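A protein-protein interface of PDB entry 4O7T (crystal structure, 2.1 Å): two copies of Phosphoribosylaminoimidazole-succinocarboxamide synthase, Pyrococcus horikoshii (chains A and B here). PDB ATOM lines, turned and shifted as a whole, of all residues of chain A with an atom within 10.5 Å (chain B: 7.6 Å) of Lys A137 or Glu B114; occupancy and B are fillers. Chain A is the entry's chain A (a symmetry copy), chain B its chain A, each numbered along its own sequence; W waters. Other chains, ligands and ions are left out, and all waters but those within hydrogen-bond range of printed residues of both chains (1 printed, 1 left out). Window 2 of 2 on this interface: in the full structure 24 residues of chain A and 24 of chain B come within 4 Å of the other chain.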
ATOM      1  N   TYR A  86      -3.446 -28.190   1.250  1.00  0.00           N
ATOM      2  CA  TYR A  86      -2.427 -28.537   0.260  1.00  0.00           C
ATOM      3  C   TYR A  86      -2.953 -29.732  -0.517  1.00  0.00           C
ATOM      4  O   TYR A  86      -3.546 -30.628   0.067  1.00  0.00           O
ATOM      5  CB  TYR A  86      -1.117 -28.913   0.936  1.00  0.00           C
ATOM      6  CG  TYR A  86      -0.412 -27.742   1.564  1.00  0.00           C
ATOM      7  CD1 TYR A  86       0.287 -26.833   0.770  1.00  0.00           C
ATOM      8  CD2 TYR A  86      -0.427 -27.548   2.939  1.00  0.00           C
ATOM      9  CE1 TYR A  86       0.956 -25.761   1.322  1.00  0.00           C
ATOM     10  CE2 TYR A  86       0.247 -26.471   3.506  1.00  0.00           C
ATOM     11  CZ  TYR A  86       0.938 -25.580   2.691  1.00  0.00           C
ATOM     12  OH  TYR A  86       1.615 -24.492   3.209  1.00  0.00           O
ATOM     13  N   PRO A  87      -2.736 -29.754  -1.840  1.00  0.00           N
ATOM     14  CA  PRO A  87      -3.170 -30.927  -2.601  1.00  0.00           C
ATOM     15  C   PRO A  87      -2.155 -32.094  -2.490  1.00  0.00           C
ATOM     16  O   PRO A  87      -1.614 -32.556  -3.510  1.00  0.00           O
ATOM     17  CB  PRO A  87      -3.275 -30.380  -4.038  1.00  0.00           C
ATOM     18  CG  PRO A  87      -2.253 -29.285  -4.093  1.00  0.00           C
ATOM     19  CD  PRO A  87      -2.188 -28.684  -2.705  1.00  0.00           C
ATOM     20  N   LEU A  88      -1.911 -32.560  -1.261  1.00  0.00           N
ATOM     21  CA  LEU A  88      -0.926 -33.616  -0.997  1.00  0.00           C
ATOM     22  C   LEU A  88      -1.445 -34.725  -0.097  1.00  0.00           C
ATOM     23  O   LEU A  88      -2.266 -34.502   0.809  1.00  0.00           O
ATOM     24  CB  LEU A  88       0.354 -33.038  -0.350  1.00  0.00           C
ATOM     25  CG  LEU A  88       1.168 -31.969  -1.108  1.00  0.00           C
ATOM     26  CD1 LEU A  88       2.201 -31.333  -0.181  1.00  0.00           C
ATOM     27  CD2 LEU A  88       1.826 -32.555  -2.348  1.00  0.00           C
ATOM     28  N   LEU A 119       5.699 -38.022  -1.081  1.00  0.00           N
ATOM     29  CA  LEU A 119       4.685 -37.035  -1.420  1.00  0.00           C
ATOM     30  C   LEU A 119       3.863 -37.540  -2.591  1.00  0.00           C
ATOM     31  O   LEU A 119       4.428 -38.009  -3.592  1.00  0.00           O
ATOM     32  CB  LEU A 119       5.329 -35.699  -1.792  1.00  0.00           C
ATOM     33  CG  LEU A 119       6.254 -35.093  -0.732  1.00  0.00           C
ATOM     34  CD1 LEU A 119       7.024 -33.909  -1.304  1.00  0.00           C
ATOM     35  CD2 LEU A 119       5.466 -34.704   0.522  1.00  0.00           C
ATOM     36  N   TYR A 121       0.579 -36.294  -5.133  1.00  0.00           N
ATOM     37  CA  TYR A 121      -0.250 -35.187  -5.567  1.00  0.00           C
ATOM     38  C   TYR A 121      -1.715 -35.657  -5.595  1.00  0.00           C
ATOM     39  O   TYR A 121      -2.049 -36.604  -6.299  1.00  0.00           O
ATOM     40  CB  TYR A 121       0.238 -34.713  -6.935  1.00  0.00           C
ATOM     41  CG  TYR A 121      -0.639 -33.682  -7.637  1.00  0.00           C
ATOM     42  CD1 TYR A 121      -1.289 -32.675  -6.918  1.00  0.00           C
ATOM     43  CD2 TYR A 121      -0.787 -33.701  -9.030  1.00  0.00           C
ATOM     44  CE1 TYR A 121      -2.063 -31.717  -7.561  1.00  0.00           C
ATOM     45  CE2 TYR A 121      -1.565 -32.747  -9.678  1.00  0.00           C
ATOM     46  CZ  TYR A 121      -2.198 -31.771  -8.933  1.00  0.00           C
ATOM     47  OH  TYR A 121      -2.958 -30.836  -9.551  1.00  0.00           O
ATOM     48  N   ILE A 131       5.061 -37.464  -6.334  1.00  0.00           N
ATOM     49  CA  ILE A 131       5.818 -36.321  -6.804  1.00  0.00           C
ATOM     50  C   ILE A 131       7.000 -36.076  -5.888  1.00  0.00           C
ATOM     51  O   ILE A 131       7.099 -36.681  -4.809  1.00  0.00           O
ATOM     52  CB  ILE A 131       4.968 -35.028  -6.877  1.00  0.00           C
ATOM     53  CG1 ILE A 131       4.312 -34.718  -5.518  1.00  0.00           C
ATOM     54  CG2 ILE A 131       3.967 -35.113  -8.029  1.00  0.00           C
ATOM     55  CD1 ILE A 131       3.850 -33.275  -5.365  1.00  0.00           C
ATOM     56  N   ASN A 132       7.889 -35.186  -6.324  1.00  0.00           N
ATOM     57  CA  ASN A 132       8.968 -34.692  -5.459  1.00  0.00           C
ATOM     58  C   ASN A 132       8.841 -33.167  -5.198  1.00  0.00           C
ATOM     59  O   ASN A 132       7.832 -32.531  -5.571  1.00  0.00           O
ATOM     60  CB  ASN A 132      10.352 -35.113  -6.007  1.00  0.00           C
ATOM     61  CG  ASN A 132      10.682 -34.467  -7.346  1.00  0.00           C
ATOM     62  OD1 ASN A 132      10.308 -33.321  -7.610  1.00  0.00           O
ATOM     63  ND2 ASN A 132      11.386 -35.199  -8.198  1.00  0.00           N
ATOM     64  N   TYR A 133       9.853 -32.582  -4.563  1.00  0.00           N
ATOM     65  CA  TYR A 133       9.828 -31.152  -4.194  1.00  0.00           C
ATOM     66  C   TYR A 133       9.724 -30.245  -5.397  1.00  0.00           C
ATOM     67  O   TYR A 133       9.196 -29.134  -5.296  1.00  0.00           O
ATOM     68  CB  TYR A 133      11.091 -30.746  -3.411  1.00  0.00           C
ATOM     69  CG  TYR A 133      11.432 -31.629  -2.232  1.00  0.00           C
ATOM     70  CD1 TYR A 133      10.466 -32.465  -1.626  1.00  0.00           C
ATOM     71  CD2 TYR A 133      12.716 -31.604  -1.683  1.00  0.00           C
ATOM     72  CE1 TYR A 133      10.789 -33.263  -0.537  1.00  0.00           C
ATOM     73  CE2 TYR A 133      13.044 -32.391  -0.590  1.00  0.00           C
ATOM     74  CZ  TYR A 133      12.085 -33.214  -0.024  1.00  0.00           C
ATOM     75  OH  TYR A 133      12.443 -33.995   1.049  1.00  0.00           O
ATOM     76  N   TYR A 134      10.265 -30.686  -6.526  1.00  0.00           N
ATOM     77  CA  TYR A 134      10.292 -29.844  -7.731  1.00  0.00           C
ATOM     78  C   TYR A 134       8.898 -29.767  -8.350  1.00  0.00           C
ATOM     79  O   TYR A 134       8.450 -28.686  -8.733  1.00  0.00           O
ATOM     80  CB  TYR A 134      11.277 -30.365  -8.770  1.00  0.00           C
ATOM     81  CG  TYR A 134      12.732 -30.268  -8.377  1.00  0.00           C
ATOM     82  CD1 TYR A 134      13.512 -29.183  -8.795  1.00  0.00           C
ATOM     83  CD2 TYR A 134      13.345 -31.270  -7.607  1.00  0.00           C
ATOM     84  CE1 TYR A 134      14.849 -29.083  -8.446  1.00  0.00           C
ATOM     85  CE2 TYR A 134      14.689 -31.174  -7.261  1.00  0.00           C
ATOM     86  CZ  TYR A 134      15.429 -30.070  -7.686  1.00  0.00           C
ATOM     87  OH  TYR A 134      16.770 -29.966  -7.373  1.00  0.00           O
ATOM     88  N   HIS A 135       8.218 -30.912  -8.452  1.00  0.00           N
ATOM     89  CA  HIS A 135       6.842 -30.915  -8.935  1.00  0.00           C
ATOM     90  C   HIS A 135       6.015 -30.066  -7.994  1.00  0.00           C
ATOM     91  O   HIS A 135       5.194 -29.265  -8.435  1.00  0.00           O
ATOM     92  CB  HIS A 135       6.237 -32.314  -8.979  1.00  0.00           C
ATOM     93  CG  HIS A 135       7.098 -33.367  -9.652  1.00  0.00           C
ATOM     94  ND1 HIS A 135       7.229 -33.459 -10.987  1.00  0.00           N
ATOM     95  CD2 HIS A 135       7.799 -34.431  -9.122  1.00  0.00           C
ATOM     96  CE1 HIS A 135       8.019 -34.506 -11.286  1.00  0.00           C
ATOM     97  NE2 HIS A 135       8.354 -35.105 -10.148  1.00  0.00           N
ATOM     98  N   ALA A 136       6.226 -30.235  -6.691  1.00  0.00           N
ATOM     99  CA  ALA A 136       5.489 -29.475  -5.686  1.00  0.00           C
ATOM    100  C   ALA A 136       5.632 -27.943  -5.882  1.00  0.00           C
ATOM    101  O   ALA A 136       4.645 -27.210  -5.852  1.00  0.00           O
ATOM    102  CB  ALA A 136       5.913 -29.892  -4.292  1.00  0.00           C
ATOM    103  N   LYS A 137       6.857 -27.482  -6.112  1.00  0.00           N
ATOM    104  CA  LYS A 137       7.095 -26.082  -6.422  1.00  0.00           C
ATOM    105  C   LYS A 137       6.259 -25.614  -7.632  1.00  0.00           C
ATOM    106  O   LYS A 137       5.638 -24.555  -7.580  1.00  0.00           O
ATOM    107  CB  LYS A 137       8.600 -25.826  -6.615  1.00  0.00           C
ATOM    108  CG  LYS A 137       8.966 -24.375  -6.925  1.00  0.00           C
ATOM    109  CD  LYS A 137       8.714 -23.485  -5.718  1.00  0.00           C
ATOM    110  CE  LYS A 137       9.058 -22.021  -5.972  1.00  0.00           C
ATOM    111  NZ  LYS A 137       8.864 -21.292  -4.681  1.00  0.00           N
ATOM    112  N   VAL A 138       6.205 -26.421  -8.691  1.00  0.00           N
ATOM    113  CA  VAL A 138       5.386 -26.080  -9.862  1.00  0.00           C
ATOM    114  C   VAL A 138       3.909 -25.978  -9.486  1.00  0.00           C
ATOM    115  O   VAL A 138       3.169 -25.171 -10.057  1.00  0.00           O
ATOM    116  CB  VAL A 138       5.576 -27.070 -11.049  1.00  0.00           C
ATOM    117  CG1 VAL A 138       4.598 -26.749 -12.189  1.00  0.00           C
ATOM    118  CG2 VAL A 138       7.005 -26.995 -11.562  1.00  0.00           C
ATOM    119  N   LEU A 139       3.494 -26.784  -8.507  1.00  0.00           N
ATOM    120  CA  LEU A 139       2.111 -26.765  -8.023  1.00  0.00           C
ATOM    121  C   LEU A 139       1.847 -25.630  -7.033  1.00  0.00           C
ATOM    122  O   LEU A 139       0.750 -25.511  -6.527  1.00  0.00           O
ATOM    123  CB  LEU A 139       1.748 -28.116  -7.399  1.00  0.00           C
ATOM    124  CG  LEU A 139       1.653 -29.287  -8.372  1.00  0.00           C
ATOM    125  CD1 LEU A 139       1.720 -30.604  -7.611  1.00  0.00           C
ATOM    126  CD2 LEU A 139       0.393 -29.204  -9.239  1.00  0.00           C
ATOM    127  N   GLY A 140       2.864 -24.807  -6.771  1.00  0.00           N
ATOM    128  CA  GLY A 140       2.732 -23.605  -5.942  1.00  0.00           C
ATOM    129  C   GLY A 140       3.126 -23.801  -4.491  1.00  0.00           C
ATOM    130  O   GLY A 140       2.771 -22.993  -3.645  1.00  0.00           O
ATOM    131  N   ILE A 141       3.855 -24.877  -4.199  1.00  0.00           N
ATOM    132  CA  ILE A 141       4.242 -25.201  -2.830  1.00  0.00           C
ATOM    133  C   ILE A 141       5.755 -25.037  -2.719  1.00  0.00           C
ATOM    134  O   ILE A 141       6.526 -25.784  -3.342  1.00  0.00           O
ATOM    135  CB  ILE A 141       3.822 -26.639  -2.418  1.00  0.00           C
ATOM    136  CG1 ILE A 141       2.377 -26.938  -2.848  1.00  0.00           C
ATOM    137  CG2 ILE A 141       3.990 -26.852  -0.918  1.00  0.00           C
ATOM    138  CD1 ILE A 141       1.995 -28.413  -2.799  1.00  0.00           C
ATOM    139  N   SER A 142       6.162 -24.049  -1.926  1.00  0.00           N
ATOM    140  CA  SER A 142       7.554 -23.666  -1.792  1.00  0.00           C
ATOM    141  C   SER A 142       8.349 -24.744  -1.084  1.00  0.00           C
ATOM    142  O   SER A 142       7.788 -25.582  -0.366  1.00  0.00           O
ATOM    143  CB  SER A 142       7.679 -22.320  -1.031  1.00  0.00           C
ATOM    144  OG  SER A 142       7.514 -22.497   0.377  1.00  0.00           O
ATOM    145  N   LEU A 143       9.662 -24.699  -1.275  1.00  0.00           N
ATOM    146  CA  LEU A 143      10.559 -25.631  -0.615  1.00  0.00           C
ATOM    147  C   LEU A 143      10.469 -25.507   0.904  1.00  0.00           C
ATOM    148  O   LEU A 143      10.469 -26.523   1.619  1.00  0.00           O
ATOM    149  CB  LEU A 143      12.005 -25.433  -1.112  1.00  0.00           C
ATOM    150  CG  LEU A 143      13.065 -26.384  -0.548  1.00  0.00           C
ATOM    151  CD1 LEU A 143      12.724 -27.835  -0.873  1.00  0.00           C
ATOM    152  CD2 LEU A 143      14.464 -26.019  -1.056  1.00  0.00           C
ATOM    153  N   ASP A 144      10.372 -24.278   1.406  1.00  0.00           N
ATOM    154  CA  ASP A 144      10.216 -24.017   2.843  1.00  0.00           C
ATOM    155  C   ASP A 144       8.987 -24.741   3.401  1.00  0.00           C
ATOM    156  O   ASP A 144       9.020 -25.348   4.474  1.00  0.00           O
ATOM    157  CB  ASP A 144      10.091 -22.504   3.078  1.00  0.00           C
ATOM    158  CG  ASP A 144       9.547 -22.160   4.453  1.00  0.00           C
ATOM    159  OD1 ASP A 144      10.278 -22.355   5.444  1.00  0.00           O
ATOM    160  OD2 ASP A 144       8.388 -21.690   4.540  1.00  0.00           O
ATOM    161  N   GLU A 145       7.890 -24.648   2.658  1.00  0.00           N
ATOM    162  CA  GLU A 145       6.637 -25.287   3.046  1.00  0.00           C
ATOM    163  C   GLU A 145       6.754 -26.817   3.070  1.00  0.00           C
ATOM    164  O   GLU A 145       6.346 -27.451   4.046  1.00  0.00           O
ATOM    165  CB  GLU A 145       5.501 -24.855   2.122  1.00  0.00           C
ATOM    166  CG  GLU A 145       4.944 -23.473   2.426  1.00  0.00           C
ATOM    167  CD  GLU A 145       4.025 -23.010   1.320  1.00  0.00           C
ATOM    168  OE1 GLU A 145       4.532 -22.633   0.251  1.00  0.00           O
ATOM    169  OE2 GLU A 145       2.801 -23.041   1.500  1.00  0.00           O
ATOM    170  N   ILE A 146       7.310 -27.395   2.001  1.00  0.00           N
ATOM    171  CA  ILE A 146       7.536 -28.852   1.930  1.00  0.00           C
ATOM    172  C   ILE A 146       8.367 -29.313   3.124  1.00  0.00           C
ATOM    173  O   ILE A 146       7.989 -30.251   3.819  1.00  0.00           O
ATOM    174  CB  ILE A 146       8.209 -29.262   0.599  1.00  0.00           C
ATOM    175  CG1 ILE A 146       7.192 -29.242  -0.553  1.00  0.00           C
ATOM    176  CG2 ILE A 146       8.854 -30.640   0.717  1.00  0.00           C
ATOM    177  CD1 ILE A 146       6.011 -30.192  -0.374  1.00  0.00           C
ATOM    178  N   LYS A 147       9.471 -28.613   3.378  1.00  0.00           N
ATOM    179  CA  LYS A 147      10.333 -28.887   4.527  1.00  0.00           C
ATOM    180  C   LYS A 147       9.614 -28.847   5.893  1.00  0.00           C
ATOM    181  O   LYS A 147       9.826 -29.736   6.715  1.00  0.00           O
ATOM    182  CB  LYS A 147      11.537 -27.932   4.539  1.00  0.00           C
ATOM    183  CG  LYS A 147      12.646 -28.334   3.581  1.00  0.00           C
ATOM    184  CD  LYS A 147      13.824 -27.375   3.659  1.00  0.00           C
ATOM    185  CE  LYS A 147      14.843 -27.666   2.564  1.00  0.00           C
ATOM    186  NZ  LYS A 147      15.637 -26.447   2.235  1.00  0.00           N
ATOM    187  N   ILE A 149       6.347 -29.253   6.309  1.00  0.00           N
ATOM    188  CA  ILE A 149       5.420 -30.400   6.209  1.00  0.00           C
ATOM    189  C   ILE A 149       6.120 -31.726   6.555  1.00  0.00           C
ATOM    190  O   ILE A 149       5.600 -32.511   7.360  1.00  0.00           O
ATOM    191  CB  ILE A 149       4.771 -30.483   4.802  1.00  0.00           C
ATOM    192  CG1 ILE A 149       3.779 -29.331   4.595  1.00  0.00           C
ATOM    193  CG2 ILE A 149       4.111 -31.840   4.569  1.00  0.00           C
ATOM    194  CD1 ILE A 149       3.392 -29.089   3.150  1.00  0.00           C
ATOM    195  N   ARG B  93      14.106 -31.495 -16.497  1.00  0.00           N
ATOM    196  CA  ARG B  93      12.981 -31.165 -17.383  1.00  0.00           C
ATOM    197  C   ARG B  93      12.695 -29.656 -17.395  1.00  0.00           C
ATOM    198  O   ARG B  93      12.546 -29.042 -16.335  1.00  0.00           O
ATOM    199  CB  ARG B  93      11.731 -31.970 -16.975  1.00  0.00           C
ATOM    200  CG  ARG B  93      12.025 -33.403 -16.481  1.00  0.00           C
ATOM    201  CD  ARG B  93      10.767 -34.222 -16.152  1.00  0.00           C
ATOM    202  NE  ARG B  93      10.125 -34.701 -17.367  1.00  0.00           N
ATOM    203  CZ  ARG B  93      10.004 -35.971 -17.756  1.00  0.00           C
ATOM    204  NH1 ARG B  93      10.428 -36.988 -16.992  1.00  0.00           N
ATOM    205  NH2 ARG B  93       9.420 -36.217 -18.936  1.00  0.00           N
ATOM    206  N   ASN B  94      12.628 -29.082 -18.597  1.00  0.00           N
ATOM    207  CA  ASN B  94      12.371 -27.646 -18.810  1.00  0.00           C
ATOM    208  C   ASN B  94      10.986 -27.390 -19.392  1.00  0.00           C
ATOM    209  O   ASN B  94      10.345 -26.390 -19.065  1.00  0.00           O
ATOM    210  CB  ASN B  94      13.429 -27.051 -19.746  1.00  0.00           C
ATOM    211  CG  ASN B  94      14.839 -27.206 -19.197  1.00  0.00           C
ATOM    212  OD1 ASN B  94      15.110 -26.809 -18.062  1.00  0.00           O
ATOM    213  ND2 ASN B  94      15.744 -27.789 -19.995  1.00  0.00           N
ATOM    214  N   VAL B  95      10.540 -28.312 -20.246  1.00  0.00           N
ATOM    215  CA  VAL B  95       9.292 -28.190 -20.984  1.00  0.00           C
ATOM    216  C   VAL B  95       8.523 -29.497 -20.759  1.00  0.00           C
ATOM    217  O   VAL B  95       9.133 -30.572 -20.787  1.00  0.00           O
ATOM    218  CB  VAL B  95       9.589 -27.963 -22.491  1.00  0.00           C
ATOM    219  CG1 VAL B  95       8.340 -28.106 -23.334  1.00  0.00           C
ATOM    220  CG2 VAL B  95      10.228 -26.590 -22.703  1.00  0.00           C
ATOM    221  N   LEU B 104       1.748 -34.073 -13.641  1.00  0.00           N
ATOM    222  CA  LEU B 104       1.275 -32.696 -13.572  1.00  0.00           C
ATOM    223  C   LEU B 104       0.198 -32.491 -14.641  1.00  0.00           C
ATOM    224  O   LEU B 104       0.378 -32.932 -15.787  1.00  0.00           O
ATOM    225  CB  LEU B 104       2.422 -31.687 -13.788  1.00  0.00           C
ATOM    226  CG  LEU B 104       3.550 -31.586 -12.745  1.00  0.00           C
ATOM    227  CD1 LEU B 104       4.642 -30.647 -13.233  1.00  0.00           C
ATOM    228  CD2 LEU B 104       3.037 -31.120 -11.392  1.00  0.00           C
ATOM    229  N   GLU B 111       5.813 -24.544 -20.786  1.00  0.00           N
ATOM    230  CA  GLU B 111       7.106 -24.090 -20.296  1.00  0.00           C
ATOM    231  C   GLU B 111       7.121 -24.039 -18.768  1.00  0.00           C
ATOM    232  O   GLU B 111       6.373 -23.260 -18.172  1.00  0.00           O
ATOM    233  CB  GLU B 111       7.393 -22.700 -20.825  1.00  0.00           C
ATOM    234  CG  GLU B 111       8.583 -22.018 -20.170  1.00  0.00           C
ATOM    235  CD  GLU B 111       9.720 -21.868 -21.143  1.00  0.00           C
ATOM    236  OE1 GLU B 111      10.078 -22.894 -21.770  1.00  0.00           O
ATOM    237  OE2 GLU B 111      10.223 -20.731 -21.301  1.00  0.00           O
ATOM    238  N   LEU B 112       7.973 -24.848 -18.139  1.00  0.00           N
ATOM    239  CA  LEU B 112       8.048 -24.861 -16.670  1.00  0.00           C
ATOM    240  C   LEU B 112       8.627 -23.560 -16.107  1.00  0.00           C
ATOM    241  O   LEU B 112       9.534 -22.991 -16.713  1.00  0.00           O
ATOM    242  CB  LEU B 112       8.845 -26.074 -16.153  1.00  0.00           C
ATOM    243  CG  LEU B 112       8.245 -27.430 -16.524  1.00  0.00           C
ATOM    244  CD1 LEU B 112       9.264 -28.543 -16.305  1.00  0.00           C
ATOM    245  CD2 LEU B 112       6.955 -27.692 -15.757  1.00  0.00           C
ATOM    246  N   PRO B 113       8.104 -23.094 -14.946  1.00  0.00           N
ATOM    247  CA  PRO B 113       8.607 -21.846 -14.353  1.00  0.00           C
ATOM    248  C   PRO B 113      10.048 -22.000 -13.882  1.00  0.00           C
ATOM    249  O   PRO B 113      10.779 -21.017 -13.793  1.00  0.00           O
ATOM    250  CB  PRO B 113       7.639 -21.580 -13.176  1.00  0.00           C
ATOM    251  CG  PRO B 113       7.015 -22.913 -12.862  1.00  0.00           C
ATOM    252  CD  PRO B 113       7.006 -23.693 -14.154  1.00  0.00           C
ATOM    253  N   GLU B 114      10.464 -23.238 -13.606  1.00  0.00           N
ATOM    254  CA  GLU B 114      11.861 -23.533 -13.298  1.00  0.00           C
ATOM    255  C   GLU B 114      12.091 -25.035 -13.538  1.00  0.00           C
ATOM    256  O   GLU B 114      11.122 -25.806 -13.589  1.00  0.00           O
ATOM    257  CB  GLU B 114      12.230 -23.129 -11.855  1.00  0.00           C
ATOM    258  CG  GLU B 114      11.526 -23.905 -10.746  1.00  0.00           C
ATOM    259  CD  GLU B 114      10.110 -23.413 -10.460  1.00  0.00           C
ATOM    260  OE1 GLU B 114       9.209 -24.259 -10.292  1.00  0.00           O
ATOM    261  OE2 GLU B 114       9.888 -22.184 -10.410  1.00  0.00           O
ATOM    262  N   PRO B 115      13.357 -25.456 -13.682  1.00  0.00           N
ATOM    263  CA  PRO B 115      13.559 -26.863 -14.052  1.00  0.00           C
ATOM    264  C   PRO B 115      13.076 -27.837 -12.973  1.00  0.00           C
ATOM    265  O   PRO B 115      13.113 -27.519 -11.779  1.00  0.00           O
ATOM    266  CB  PRO B 115      15.078 -26.962 -14.246  1.00  0.00           C
ATOM    267  CG  PRO B 115      15.537 -25.537 -14.471  1.00  0.00           C
ATOM    268  CD  PRO B 115      14.632 -24.711 -13.605  1.00  0.00           C
ATOM    269  N   ILE B 116      12.611 -29.009 -13.403  1.00  0.00           N
ATOM    270  CA  ILE B 116      12.275 -30.108 -12.494  1.00  0.00           C
ATOM    271  C   ILE B 116      13.365 -31.185 -12.568  1.00  0.00           C
ATOM    272  O   ILE B 116      13.787 -31.567 -13.656  1.00  0.00           O
ATOM    273  CB  ILE B 116      10.923 -30.737 -12.869  1.00  0.00           C
ATOM    274  CG1 ILE B 116       9.788 -29.778 -12.514  1.00  0.00           C
ATOM    275  CG2 ILE B 116      10.743 -32.095 -12.183  1.00  0.00           C
ATOM    276  CD1 ILE B 116       8.437 -30.222 -13.040  1.00  0.00           C
ATOM    277  N   VAL B 117      13.826 -31.659 -11.415  1.00  0.00           N
ATOM    278  CA  VAL B 117      14.781 -32.777 -11.375  1.00  0.00           C
ATOM    279  C   VAL B 117      14.033 -33.976 -10.824  1.00  0.00           C
ATOM    280  O   VAL B 117      13.370 -33.874  -9.792  1.00  0.00           O
ATOM    281  CB  VAL B 117      16.020 -32.475 -10.493  1.00  0.00           C
ATOM    282  CG1 VAL B 117      17.053 -33.588 -10.619  1.00  0.00           C
ATOM    283  CG2 VAL B 117      16.649 -31.148 -10.902  1.00  0.00           C
ATOM    284  N   LEU B 154      21.670 -29.631 -12.726  1.00  0.00           N
ATOM    285  CA  LEU B 154      21.080 -28.325 -12.998  1.00  0.00           C
ATOM    286  C   LEU B 154      22.057 -27.393 -13.704  1.00  0.00           C
ATOM    287  O   LEU B 154      21.649 -26.567 -14.539  1.00  0.00           O
ATOM    288  CB  LEU B 154      20.580 -27.699 -11.700  1.00  0.00           C
ATOM    289  CG  LEU B 154      19.271 -28.282 -11.168  1.00  0.00           C
ATOM    290  CD1 LEU B 154      18.978 -27.741  -9.773  1.00  0.00           C
ATOM    291  CD2 LEU B 154      18.120 -27.980 -12.129  1.00  0.00           C
ATOM    292  N   ASN B 157      22.156 -28.715 -17.226  1.00  0.00           N
ATOM    293  CA  ASN B 157      20.961 -28.156 -17.866  1.00  0.00           C
ATOM    294  C   ASN B 157      21.207 -26.748 -18.427  1.00  0.00           C
ATOM    295  O   ASN B 157      20.966 -26.500 -19.605  1.00  0.00           O
ATOM    296  CB  ASN B 157      19.804 -28.111 -16.876  1.00  0.00           C
ATOM    297  CG  ASN B 157      18.479 -27.750 -17.531  1.00  0.00           C
ATOM    298  OD1 ASN B 157      18.185 -28.169 -18.660  1.00  0.00           O
ATOM    299  ND2 ASN B 157      17.661 -26.979 -16.813  1.00  0.00           N
HETATM  300  O   HOH W   1      14.371 -34.619  -7.193  1.00  0.00           O
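Of the printed residues of chain B, Asn A132 touches Val B117 (2.9 Å).
Of the printed residues of chain B, Val A138 touches Glu B114 and Ile B116.
Of the printed residues of chain B, Leu A139 touches Leu B104.
No residue of chain A comes within 4 Å of Leu B112.
Glu B114 touches just these residues of chain A: Lys A137 and Val A138.
Of the printed residues of chain A, Ile B116 touches Tyr A134 (3.9 Å), His A135 (3.7 Å) and Val A138 (3.8 Å).
Printed residues of chain A within 4 Å of Leu B154: Tyr A134.
The nearest residue of chain B that does not touch Lys A137 is Pro B113 (5.7 Å).
The nearest printed residue of chain B that does not touch Leu A139 is Glu B114 (6.5 Å).
Printed residues of chain B that touch a printed residue of chain A: Leu B104, Glu B114, Pro B115, Ile B116, Val B117 and Leu B154.
Hydrophobic or aromatic side chains of chain B that line the printed part of chain A: Leu B104, Ile B116, Val B117 and Leu B154.
Along chain B the printed residues that touch a printed residue of chain A span positions 104 to 154.
Printed residues of chain A that touch a printed residue of chain B: Asn A132, Tyr A134, His A135, Lys A137, Val A138 and Leu A139.
Hydrophobic or aromatic side chains of chain A that line the printed part of chain B: Tyr A134, His A135, Val A138 and Leu A139.
Among the printed residues, 10 pairs touch across the chains.
Among the printed residues, no Asp or Glu carboxylate lies within 4 Å of a Lys or Arg side-chain nitrogen of the other chain.
Water W1 lies within hydrogen-bond range of O of Val B117 (2.9 Å) and ND2 of Asn A132 (3.2 Å).
Among the printed residues, pairs that only touch across the chains: Lys A137 with Glu B114 (3.4 Å), Tyr A134 with Val B117 (3.4 Å), Tyr A134 with Pro B115 (3.4 Å), Val A138 with Glu B114 (3.7 Å), His A135 with Ile B116 (3.7 Å), Leu A139 with Leu B104 (3.8 Å), Val A138 with Ile B116 (3.8 Å), Tyr A134 with Ile B116 (3.9 Å) and Tyr A134 with Leu B154 (3.9 Å).
ND2 of Asn A132 is in hydrogen-bond range of O of Val B117 (2.9 Å).
No position is printed for both chains.
Of the 10 pairs that touch across the chains among the printed residues, none has its exchanged pair printed and touching as well.
The backbone carbonyl oxygen (O) of Ile B116 sits at hydrogen-bond distance from the backbone NH (N) of Arg B93 (2.9 Å).
OD1 of Asn A132 is in hydrogen-bond range of N of Tyr A134 (2.8 Å).
The side-chain amide oxygen (OD1) of Asn A132 lies close to the backbone NH (N) of His A135 (3.3 Å).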
